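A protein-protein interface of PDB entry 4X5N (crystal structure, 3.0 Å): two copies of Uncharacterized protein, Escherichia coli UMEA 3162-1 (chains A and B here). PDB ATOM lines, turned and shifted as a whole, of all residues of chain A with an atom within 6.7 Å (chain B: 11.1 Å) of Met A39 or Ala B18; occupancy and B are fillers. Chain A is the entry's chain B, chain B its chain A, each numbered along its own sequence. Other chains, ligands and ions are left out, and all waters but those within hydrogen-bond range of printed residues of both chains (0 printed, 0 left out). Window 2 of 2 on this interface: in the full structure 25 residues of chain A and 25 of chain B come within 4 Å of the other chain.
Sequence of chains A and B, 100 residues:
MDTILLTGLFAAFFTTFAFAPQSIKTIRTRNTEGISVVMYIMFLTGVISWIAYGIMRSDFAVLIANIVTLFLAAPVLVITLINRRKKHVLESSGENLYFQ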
ATOM      1  N   GLY A  34     -16.669  -9.669 -32.123  1.00  0.00           N
ATOM      2  CA  GLY A  34     -16.091  -9.143 -30.901  1.00  0.00           C
ATOM      3  C   GLY A  34     -14.590  -9.342 -30.805  1.00  0.00           C
ATOM      4  O   GLY A  34     -13.966  -8.952 -29.818  1.00  0.00           O
ATOM      5  N   ILE A  35     -14.008  -9.943 -31.836  1.00  0.00           N
ATOM      6  CA  ILE A  35     -12.595 -10.300 -31.813  1.00  0.00           C
ATOM      7  C   ILE A  35     -11.697  -9.072 -31.885  1.00  0.00           C
ATOM      8  O   ILE A  35     -11.922  -8.174 -32.697  1.00  0.00           O
ATOM      9  CB  ILE A  35     -12.244 -11.249 -32.973  1.00  0.00           C
ATOM     10  CG1 ILE A  35     -13.234 -12.412 -33.024  1.00  0.00           C
ATOM     11  CG2 ILE A  35     -10.820 -11.768 -32.840  1.00  0.00           C
ATOM     12  CD1 ILE A  35     -13.289 -13.233 -31.755  1.00  0.00           C
ATOM     13  N   SER A  36     -10.683  -9.043 -31.025  1.00  0.00           N
ATOM     14  CA  SER A  36      -9.692  -7.974 -31.031  1.00  0.00           C
ATOM     15  C   SER A  36      -8.487  -8.364 -31.875  1.00  0.00           C
ATOM     16  O   SER A  36      -7.819  -9.358 -31.589  1.00  0.00           O
ATOM     17  CB  SER A  36      -9.245  -7.643 -29.607  1.00  0.00           C
ATOM     18  OG  SER A  36      -8.184  -6.709 -29.611  1.00  0.00           O
ATOM     19  N   VAL A  37      -8.211  -7.579 -32.911  1.00  0.00           N
ATOM     20  CA  VAL A  37      -7.071  -7.840 -33.783  1.00  0.00           C
ATOM     21  C   VAL A  37      -5.755  -7.754 -33.011  1.00  0.00           C
ATOM     22  O   VAL A  37      -4.905  -8.642 -33.120  1.00  0.00           O
ATOM     23  CB  VAL A  37      -7.026  -6.854 -34.964  1.00  0.00           C
ATOM     24  CG1 VAL A  37      -5.935  -7.254 -35.950  1.00  0.00           C
ATOM     25  CG2 VAL A  37      -8.380  -6.793 -35.654  1.00  0.00           C
ATOM     26  N   VAL A  38      -5.605  -6.690 -32.226  1.00  0.00           N
ATOM     27  CA  VAL A  38      -4.381  -6.436 -31.477  1.00  0.00           C
ATOM     28  C   VAL A  38      -4.096  -7.526 -30.450  1.00  0.00           C
ATOM     29  O   VAL A  38      -2.950  -7.955 -30.299  1.00  0.00           O
ATOM     30  CB  VAL A  38      -4.439  -5.082 -30.748  1.00  0.00           C
ATOM     31  CG1 VAL A  38      -3.065  -4.716 -30.216  1.00  0.00           C
ATOM     32  CG2 VAL A  38      -4.955  -3.996 -31.676  1.00  0.00           C
ATOM     33  N   MET A  39      -5.136  -7.973 -29.750  1.00  0.00           N
ATOM     34  CA  MET A  39      -4.968  -8.979 -28.704  1.00  0.00           C
ATOM     35  C   MET A  39      -4.546 -10.333 -29.273  1.00  0.00           C
ATOM     36  O   MET A  39      -3.885 -11.116 -28.593  1.00  0.00           O
ATOM     37  CB  MET A  39      -6.255  -9.123 -27.878  1.00  0.00           C
ATOM     38  CG  MET A  39      -6.431  -8.043 -26.815  1.00  0.00           C
ATOM     39  SD  MET A  39      -7.500  -8.515 -25.432  1.00  0.00           S
ATOM     40  CE  MET A  39      -9.127  -8.175 -26.097  1.00  0.00           C
ATOM     41  N   TYR A  40      -4.920 -10.605 -30.520  1.00  0.00           N
ATOM     42  CA  TYR A  40      -4.516 -11.847 -31.173  1.00  0.00           C
ATOM     43  C   TYR A  40      -3.079 -11.752 -31.690  1.00  0.00           C
ATOM     44  O   TYR A  40      -2.341 -12.738 -31.678  1.00  0.00           O
ATOM     45  CB  TYR A  40      -5.469 -12.204 -32.319  1.00  0.00           C
ATOM     46  CG  TYR A  40      -6.386 -13.374 -32.022  1.00  0.00           C
ATOM     47  CD1 TYR A  40      -5.906 -14.679 -32.021  1.00  0.00           C
ATOM     48  CD2 TYR A  40      -7.734 -13.176 -31.755  1.00  0.00           C
ATOM     49  CE1 TYR A  40      -6.743 -15.751 -31.755  1.00  0.00           C
ATOM     50  CE2 TYR A  40      -8.578 -14.242 -31.488  1.00  0.00           C
ATOM     51  CZ  TYR A  40      -8.076 -15.526 -31.490  1.00  0.00           C
ATOM     52  OH  TYR A  40      -8.912 -16.588 -31.226  1.00  0.00           O
ATOM     53  N   ILE A  41      -2.694 -10.562 -32.144  1.00  0.00           N
ATOM     54  CA  ILE A  41      -1.334 -10.320 -32.618  1.00  0.00           C
ATOM     55  C   ILE A  41      -0.316 -10.616 -31.511  1.00  0.00           C
ATOM     56  O   ILE A  41       0.639 -11.368 -31.721  1.00  0.00           O
ATOM     57  CB  ILE A  41      -1.163  -8.868 -33.119  1.00  0.00           C
ATOM     58  CG1 ILE A  41      -2.018  -8.621 -34.365  1.00  0.00           C
ATOM     59  CG2 ILE A  41       0.298  -8.569 -33.421  1.00  0.00           C
ATOM     60  CD1 ILE A  41      -1.492  -9.292 -35.620  1.00  0.00           C
ATOM     61  N   MET A  42      -0.537 -10.033 -30.334  1.00  0.00           N
ATOM     62  CA  MET A  42       0.291 -10.296 -29.158  1.00  0.00           C
ATOM     63  C   MET A  42       0.345 -11.785 -28.830  1.00  0.00           C
ATOM     64  O   MET A  42       1.422 -12.352 -28.629  1.00  0.00           O
ATOM     65  CB  MET A  42      -0.240  -9.530 -27.942  1.00  0.00           C
ATOM     66  CG  MET A  42      -0.430  -8.040 -28.158  1.00  0.00           C
ATOM     67  SD  MET A  42      -1.030  -7.207 -26.671  1.00  0.00           S
ATOM     68  CE  MET A  42       0.173  -7.767 -25.467  1.00  0.00           C
ATOM     69  N   PHE A  43      -0.834 -12.401 -28.768  1.00  0.00           N
ATOM     70  CA  PHE A  43      -0.978 -13.818 -28.446  1.00  0.00           C
ATOM     71  C   PHE A  43      -0.151 -14.688 -29.378  1.00  0.00           C
ATOM     72  O   PHE A  43       0.528 -15.617 -28.936  1.00  0.00           O
ATOM     73  CB  PHE A  43      -2.449 -14.225 -28.529  1.00  0.00           C
ATOM     74  CG  PHE A  43      -2.724 -15.627 -28.068  1.00  0.00           C
ATOM     75  CD1 PHE A  43      -2.980 -15.885 -26.731  1.00  0.00           C
ATOM     76  CD2 PHE A  43      -2.746 -16.683 -28.968  1.00  0.00           C
ATOM     77  CE1 PHE A  43      -3.242 -17.170 -26.294  1.00  0.00           C
ATOM     78  CE2 PHE A  43      -3.006 -17.971 -28.536  1.00  0.00           C
ATOM     79  CZ  PHE A  43      -3.255 -18.213 -27.197  1.00  0.00           C
ATOM     80  N   LEU A  44      -0.217 -14.381 -30.669  1.00  0.00           N
ATOM     81  CA  LEU A  44       0.520 -15.141 -31.667  1.00  0.00           C
ATOM     82  C   LEU A  44       2.020 -14.886 -31.542  1.00  0.00           C
ATOM     83  O   LEU A  44       2.822 -15.787 -31.781  1.00  0.00           O
ATOM     84  CB  LEU A  44       0.026 -14.805 -33.075  1.00  0.00           C
ATOM     85  CG  LEU A  44      -1.063 -15.726 -33.635  1.00  0.00           C
ATOM     86  CD1 LEU A  44      -2.290 -15.751 -32.736  1.00  0.00           C
ATOM     87  CD2 LEU A  44      -1.450 -15.327 -35.052  1.00  0.00           C
ATOM     88  N   LEU B   9      10.517 -15.855 -21.157  1.00  0.00           N
ATOM     89  CA  LEU B   9       9.778 -14.814 -20.451  1.00  0.00           C
ATOM     90  C   LEU B   9       9.079 -13.878 -21.435  1.00  0.00           C
ATOM     91  O   LEU B   9       7.966 -13.418 -21.181  1.00  0.00           O
ATOM     92  CB  LEU B   9      10.706 -14.024 -19.527  1.00  0.00           C
ATOM     93  CG  LEU B   9      11.252 -14.781 -18.312  1.00  0.00           C
ATOM     94  CD1 LEU B   9      12.128 -13.881 -17.450  1.00  0.00           C
ATOM     95  CD2 LEU B   9      10.120 -15.374 -17.488  1.00  0.00           C
ATOM     96  N   PHE B  10       9.739 -13.605 -22.556  1.00  0.00           N
ATOM     97  CA  PHE B  10       9.139 -12.824 -23.631  1.00  0.00           C
ATOM     98  C   PHE B  10       7.915 -13.548 -24.176  1.00  0.00           C
ATOM     99  O   PHE B  10       6.879 -12.935 -24.440  1.00  0.00           O
ATOM    100  CB  PHE B  10      10.154 -12.580 -24.749  1.00  0.00           C
ATOM    101  CG  PHE B  10       9.616 -11.771 -25.890  1.00  0.00           C
ATOM    102  CD1 PHE B  10       9.663 -10.387 -25.855  1.00  0.00           C
ATOM    103  CD2 PHE B  10       9.068 -12.394 -27.002  1.00  0.00           C
ATOM    104  CE1 PHE B  10       9.169  -9.638 -26.908  1.00  0.00           C
ATOM    105  CE2 PHE B  10       8.572 -11.650 -28.058  1.00  0.00           C
ATOM    106  CZ  PHE B  10       8.623 -10.272 -28.011  1.00  0.00           C
ATOM    107  N   ALA B  11       8.049 -14.859 -24.347  1.00  0.00           N
ATOM    108  CA  ALA B  11       6.943 -15.695 -24.794  1.00  0.00           C
ATOM    109  C   ALA B  11       5.847 -15.751 -23.735  1.00  0.00           C
ATOM    110  O   ALA B  11       4.659 -15.656 -24.049  1.00  0.00           O
ATOM    111  CB  ALA B  11       7.433 -17.093 -25.123  1.00  0.00           C
ATOM    112  N   ALA B  12       6.260 -15.916 -22.481  1.00  0.00           N
ATOM    113  CA  ALA B  12       5.328 -15.975 -21.361  1.00  0.00           C
ATOM    114  C   ALA B  12       4.488 -14.705 -21.262  1.00  0.00           C
ATOM    115  O   ALA B  12       3.261 -14.777 -21.235  1.00  0.00           O
ATOM    116  CB  ALA B  12       6.078 -16.213 -20.061  1.00  0.00           C
ATOM    117  N   PHE B  13       5.154 -13.551 -21.220  1.00  0.00           N
ATOM    118  CA  PHE B  13       4.481 -12.259 -21.058  1.00  0.00           C
ATOM    119  C   PHE B  13       3.353 -12.045 -22.065  1.00  0.00           C
ATOM    120  O   PHE B  13       2.252 -11.640 -21.695  1.00  0.00           O
ATOM    121  CB  PHE B  13       5.495 -11.117 -21.180  1.00  0.00           C
ATOM    122  CG  PHE B  13       4.889  -9.743 -21.050  1.00  0.00           C
ATOM    123  CD1 PHE B  13       4.649  -9.195 -19.801  1.00  0.00           C
ATOM    124  CD2 PHE B  13       4.573  -8.995 -22.176  1.00  0.00           C
ATOM    125  CE1 PHE B  13       4.095  -7.931 -19.677  1.00  0.00           C
ATOM    126  CE2 PHE B  13       4.019  -7.733 -22.057  1.00  0.00           C
ATOM    127  CZ  PHE B  13       3.782  -7.201 -20.807  1.00  0.00           C
ATOM    128  N   PHE B  14       3.632 -12.320 -23.335  1.00  0.00           N
ATOM    129  CA  PHE B  14       2.668 -12.066 -24.400  1.00  0.00           C
ATOM    130  C   PHE B  14       1.467 -13.015 -24.357  1.00  0.00           C
ATOM    131  O   PHE B  14       0.332 -12.579 -24.522  1.00  0.00           O
ATOM    132  CB  PHE B  14       3.349 -12.149 -25.766  1.00  0.00           C
ATOM    133  CG  PHE B  14       3.957 -10.850 -26.223  1.00  0.00           C
ATOM    134  CD1 PHE B  14       3.220  -9.958 -26.986  1.00  0.00           C
ATOM    135  CD2 PHE B  14       5.266 -10.522 -25.898  1.00  0.00           C
ATOM    136  CE1 PHE B  14       3.775  -8.765 -27.413  1.00  0.00           C
ATOM    137  CE2 PHE B  14       5.824  -9.329 -26.321  1.00  0.00           C
ATOM    138  CZ  PHE B  14       5.079  -8.451 -27.079  1.00  0.00           C
ATOM    139  N   THR B  15       1.713 -14.304 -24.136  1.00  0.00           N
ATOM    140  CA  THR B  15       0.637 -15.299 -24.116  1.00  0.00           C
ATOM    141  C   THR B  15      -0.308 -15.152 -22.922  1.00  0.00           C
ATOM    142  O   THR B  15      -1.525 -15.256 -23.079  1.00  0.00           O
ATOM    143  CB  THR B  15       1.205 -16.731 -24.113  1.00  0.00           C
ATOM    144  OG1 THR B  15       2.516 -16.724 -23.532  1.00  0.00           O
ATOM    145  CG2 THR B  15       1.289 -17.277 -25.534  1.00  0.00           C
ATOM    146  N   THR B  16       0.244 -14.905 -21.735  1.00  0.00           N
ATOM    147  CA  THR B  16      -0.580 -14.835 -20.528  1.00  0.00           C
ATOM    148  C   THR B  16      -1.224 -13.464 -20.316  1.00  0.00           C
ATOM    149  O   THR B  16      -2.216 -13.352 -19.602  1.00  0.00           O
ATOM    150  CB  THR B  16       0.232 -15.200 -19.261  1.00  0.00           C
ATOM    151  OG1 THR B  16      -0.655 -15.326 -18.141  1.00  0.00           O
ATOM    152  CG2 THR B  16       1.267 -14.129 -18.953  1.00  0.00           C
ATOM    153  N   PHE B  17      -0.674 -12.426 -20.939  1.00  0.00           N
ATOM    154  CA  PHE B  17      -1.186 -11.073 -20.727  1.00  0.00           C
ATOM    155  C   PHE B  17      -1.865 -10.469 -21.959  1.00  0.00           C
ATOM    156  O   PHE B  17      -2.301  -9.318 -21.924  1.00  0.00           O
ATOM    157  CB  PHE B  17      -0.060 -10.141 -20.264  1.00  0.00           C
ATOM    158  CG  PHE B  17       0.237 -10.223 -18.789  1.00  0.00           C
ATOM    159  CD1 PHE B  17      -0.786 -10.401 -17.872  1.00  0.00           C
ATOM    160  CD2 PHE B  17       1.540 -10.113 -18.320  1.00  0.00           C
ATOM    161  CE1 PHE B  17      -0.514 -10.472 -16.514  1.00  0.00           C
ATOM    162  CE2 PHE B  17       1.815 -10.183 -16.963  1.00  0.00           C
ATOM    163  CZ  PHE B  17       0.786 -10.362 -16.062  1.00  0.00           C
ATOM    164  N   ALA B  18      -1.955 -11.234 -23.044  1.00  0.00           N
ATOM    165  CA  ALA B  18      -2.659 -10.761 -24.234  1.00  0.00           C
ATOM    166  C   ALA B  18      -4.148 -10.613 -23.950  1.00  0.00           C
ATOM    167  O   ALA B  18      -4.745  -9.579 -24.246  1.00  0.00           O
ATOM    168  CB  ALA B  18      -2.444 -11.705 -25.404  1.00  0.00           C
ATOM    169  N   PHE B  19      -4.738 -11.655 -23.370  1.00  0.00           N
ATOM    170  CA  PHE B  19      -6.172 -11.682 -23.113  1.00  0.00           C
ATOM    171  C   PHE B  19      -6.497 -11.505 -21.627  1.00  0.00           C
ATOM    172  O   PHE B  19      -7.636 -11.713 -21.204  1.00  0.00           O
ATOM    173  CB  PHE B  19      -6.778 -12.986 -23.636  1.00  0.00           C
ATOM    174  CG  PHE B  19      -7.084 -12.967 -25.111  1.00  0.00           C
ATOM    175  CD1 PHE B  19      -8.260 -12.401 -25.577  1.00  0.00           C
ATOM    176  CD2 PHE B  19      -6.201 -13.522 -26.032  1.00  0.00           C
ATOM    177  CE1 PHE B  19      -8.551 -12.383 -26.935  1.00  0.00           C
ATOM    178  CE2 PHE B  19      -6.484 -13.507 -27.390  1.00  0.00           C
ATOM    179  CZ  PHE B  19      -7.660 -12.937 -27.842  1.00  0.00           C
ATOM    180  N   ALA B  20      -5.493 -11.119 -20.842  1.00  0.00           N
ATOM    181  CA  ALA B  20      -5.695 -10.801 -19.426  1.00  0.00           C
ATOM    182  C   ALA B  20      -6.700  -9.665 -19.172  1.00  0.00           C
ATOM    183  O   ALA B  20      -7.470  -9.746 -18.216  1.00  0.00           O
ATOM    184  CB  ALA B  20      -4.352 -10.467 -18.764  1.00  0.00           C
ATOM    185  N   PRO B  21      -6.689  -8.597 -20.004  1.00  0.00           N
ATOM    186  CA  PRO B  21      -7.693  -7.543 -19.802  1.00  0.00           C
ATOM    187  C   PRO B  21      -9.138  -8.033 -19.811  1.00  0.00           C
ATOM    188  O   PRO B  21      -9.965  -7.498 -19.073  1.00  0.00           O
ATOM    189  CB  PRO B  21      -7.451  -6.606 -20.988  1.00  0.00           C
ATOM    190  CG  PRO B  21      -6.021  -6.752 -21.270  1.00  0.00           C
ATOM    191  CD  PRO B  21      -5.688  -8.185 -21.007  1.00  0.00           C
ATOM    192  N   GLN B  22      -9.437  -9.032 -20.634  1.00  0.00           N
ATOM    193  CA  GLN B  22     -10.799  -9.538 -20.728  1.00  0.00           C
ATOM    194  C   GLN B  22     -11.211 -10.271 -19.452  1.00  0.00           C
ATOM    195  O   GLN B  22     -12.349 -10.145 -19.000  1.00  0.00           O
ATOM    196  CB  GLN B  22     -10.948 -10.451 -21.946  1.00  0.00           C
ATOM    197  CG  GLN B  22     -12.050 -10.015 -22.898  1.00  0.00           C
ATOM    198  CD  GLN B  22     -11.918 -10.634 -24.271  1.00  0.00           C
ATOM    199  OE1 GLN B  22     -11.203 -11.617 -24.456  1.00  0.00           O
ATOM    200  NE2 GLN B  22     -12.605 -10.052 -25.249  1.00  0.00           N
ATOM    201  N   SER B  23     -10.283 -11.023 -18.868  1.00  0.00           N
ATOM    202  CA  SER B  23     -10.567 -11.742 -17.632  1.00  0.00           C
ATOM    203  C   SER B  23     -10.727 -10.780 -16.453  1.00  0.00           C
ATOM    204  O   SER B  23     -11.672 -10.903 -15.674  1.00  0.00           O
ATOM    205  CB  SER B  23      -9.471 -12.769 -17.344  1.00  0.00           C
ATOM    206  OG  SER B  23      -9.609 -13.904 -18.185  1.00  0.00           O
ATOM    207  N   ILE B  24      -9.810  -9.822 -16.333  1.00  0.00           N
ATOM    208  CA  ILE B  24      -9.896  -8.778 -15.308  1.00  0.00           C
ATOM    209  C   ILE B  24     -11.203  -7.998 -15.431  1.00  0.00           C
ATOM    210  O   ILE B  24     -11.851  -7.678 -14.432  1.00  0.00           O
ATOM    211  CB  ILE B  24      -8.707  -7.792 -15.402  1.00  0.00           C
ATOM    212  CG1 ILE B  24      -7.400  -8.475 -14.976  1.00  0.00           C
ATOM    213  CG2 ILE B  24      -8.970  -6.535 -14.569  1.00  0.00           C
ATOM    214  CD1 ILE B  24      -6.840  -7.989 -13.642  1.00  0.00           C
ATOM    215  N   LYS B  25     -11.577  -7.696 -16.669  1.00  0.00           N
ATOM    216  CA  LYS B  25     -12.848  -7.050 -16.956  1.00  0.00           C
ATOM    217  C   LYS B  25     -14.009  -7.887 -16.426  1.00  0.00           C
ATOM    218  O   LYS B  25     -14.868  -7.381 -15.704  1.00  0.00           O
ATOM    219  CB  LYS B  25     -13.005  -6.822 -18.461  1.00  0.00           C
ATOM    220  CG  LYS B  25     -14.325  -6.179 -18.846  1.00  0.00           C
ATOM    221  CD  LYS B  25     -14.513  -6.168 -20.353  1.00  0.00           C
ATOM    222  CE  LYS B  25     -15.762  -5.394 -20.742  1.00  0.00           C
ATOM    223  NZ  LYS B  25     -16.985  -5.970 -20.125  1.00  0.00           N
ATOM    224  N   THR B  26     -14.009  -9.171 -16.781  1.00  0.00           N
ATOM    225  CA  THR B  26     -15.091 -10.090 -16.435  1.00  0.00           C
ATOM    226  C   THR B  26     -15.176 -10.328 -14.932  1.00  0.00           C
ATOM    227  O   THR B  26     -16.262 -10.517 -14.383  1.00  0.00           O
ATOM    228  CB  THR B  26     -14.915 -11.444 -17.139  1.00  0.00           C
ATOM    229  OG1 THR B  26     -14.253 -11.256 -18.395  1.00  0.00           O
ATOM    230  CG2 THR B  26     -16.267 -12.106 -17.367  1.00  0.00           C
ATOM    231  N   ALA B  65       4.316 -18.649 -15.799  1.00  0.00           N
ATOM    232  CA  ALA B  65       3.339 -18.323 -16.825  1.00  0.00           C
ATOM    233  C   ALA B  65       2.004 -18.944 -16.459  1.00  0.00           C
ATOM    234  O   ALA B  65       0.966 -18.292 -16.526  1.00  0.00           O
ATOM    235  CB  ALA B  65       3.801 -18.809 -18.190  1.00  0.00           C
ATOM    236  N   VAL B  68       0.525 -17.367 -12.876  1.00  0.00           N
ATOM    237  CA  VAL B  68      -0.251 -16.150 -13.060  1.00  0.00           C
ATOM    238  C   VAL B  68      -1.560 -16.441 -13.786  1.00  0.00           C
ATOM    239  O   VAL B  68      -2.625 -16.011 -13.343  1.00  0.00           O
ATOM    240  CB  VAL B  68       0.552 -15.091 -13.839  1.00  0.00           C
ATOM    241  CG1 VAL B  68      -0.317 -13.887 -14.153  1.00  0.00           C
ATOM    242  CG2 VAL B  68       1.785 -14.676 -13.048  1.00  0.00           C
ATOM    243  N   THR B  69      -1.476 -17.194 -14.882  1.00  0.00           N
ATOM    244  CA  THR B  69      -2.658 -17.552 -15.667  1.00  0.00           C
ATOM    245  C   THR B  69      -3.730 -18.235 -14.814  1.00  0.00           C
ATOM    246  O   THR B  69      -4.915 -18.183 -15.141  1.00  0.00           O
ATOM    247  CB  THR B  69      -2.301 -18.484 -16.850  1.00  0.00           C
ATOM    248  OG1 THR B  69      -1.045 -18.092 -17.417  1.00  0.00           O
ATOM    249  CG2 THR B  69      -3.380 -18.427 -17.926  1.00  0.00           C
ATOM    250  N   LEU B  72      -5.922 -15.629 -13.133  1.00  0.00           N
ATOM    251  CA  LEU B  72      -6.810 -14.932 -14.058  1.00  0.00           C
ATOM    252  C   LEU B  72      -8.053 -15.769 -14.302  1.00  0.00           C
ATOM    253  O   LEU B  72      -9.148 -15.241 -14.478  1.00  0.00           O
ATOM    254  CB  LEU B  72      -6.113 -14.641 -15.391  1.00  0.00           C
ATOM    255  CG  LEU B  72      -5.262 -13.377 -15.532  1.00  0.00           C
ATOM    256  CD1 LEU B  72      -5.936 -12.193 -14.855  1.00  0.00           C
ATOM    257  CD2 LEU B  72      -3.856 -13.590 -14.998  1.00  0.00           C
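O of Ala B12 lies within hydrogen-bond range of OG1 of Thr B15, at 3.1 Å. O of Ala B11 is in hydrogen-bond range of OG1 of Thr B15, 2.4 Å away. The side-chain hydroxyl of Ser A36 is in hydrogen-bond range of the backbone NH of Met A39, 3.3 Å away.
No position is printed for both chains.
The side-chain sulfur of Met A39 sits close to the backbone carbonyl oxygen of Ala B18 (3.2 Å).
Of the printed residues of chain A, Ala B18 touches Met A39 (3.2 Å) and Phe A43 (3.8 Å). No residue of chain B comes within 4 Å of Val A37. Val A38 touches none of the printed residues of chain B. Phe A43 touches just these residues of chain B: Thr B15 and Ala B18. Printed residues of chain A within 4 Å of Thr B15: Phe A43. Printed residues of chain A within 4 Å of Phe B19: Met A39 and Tyr A40. The nearest printed residue of chain A that does not touch Ala B18 is Met A42 (4.004 Å). The nearest printed residue of chain A that does not touch Thr B15 is Met A42 (4.9 Å).
CE2 of Phe B19 touches O of Met A39, 3.7 Å away. Tyr A40 touches Phe B19 (CD2 to CZ, 3.9 Å). Met A42 touches Phe B14. O of Phe A43 touches CG2 of Thr B15, at 3.9 Å. N of Phe A43 touches CB of Ala B18, at 3.8 Å.
Of the 11 printed residues of chain A, 4 touch a printed residue of chain B. Of the 22 printed residues of chain B, 4 touch a printed residue of chain A. Hydrophobic or aromatic side chains of chain B within 4 Å of the printed part of chain A: Phe B14, Ala B18 and Phe B19.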
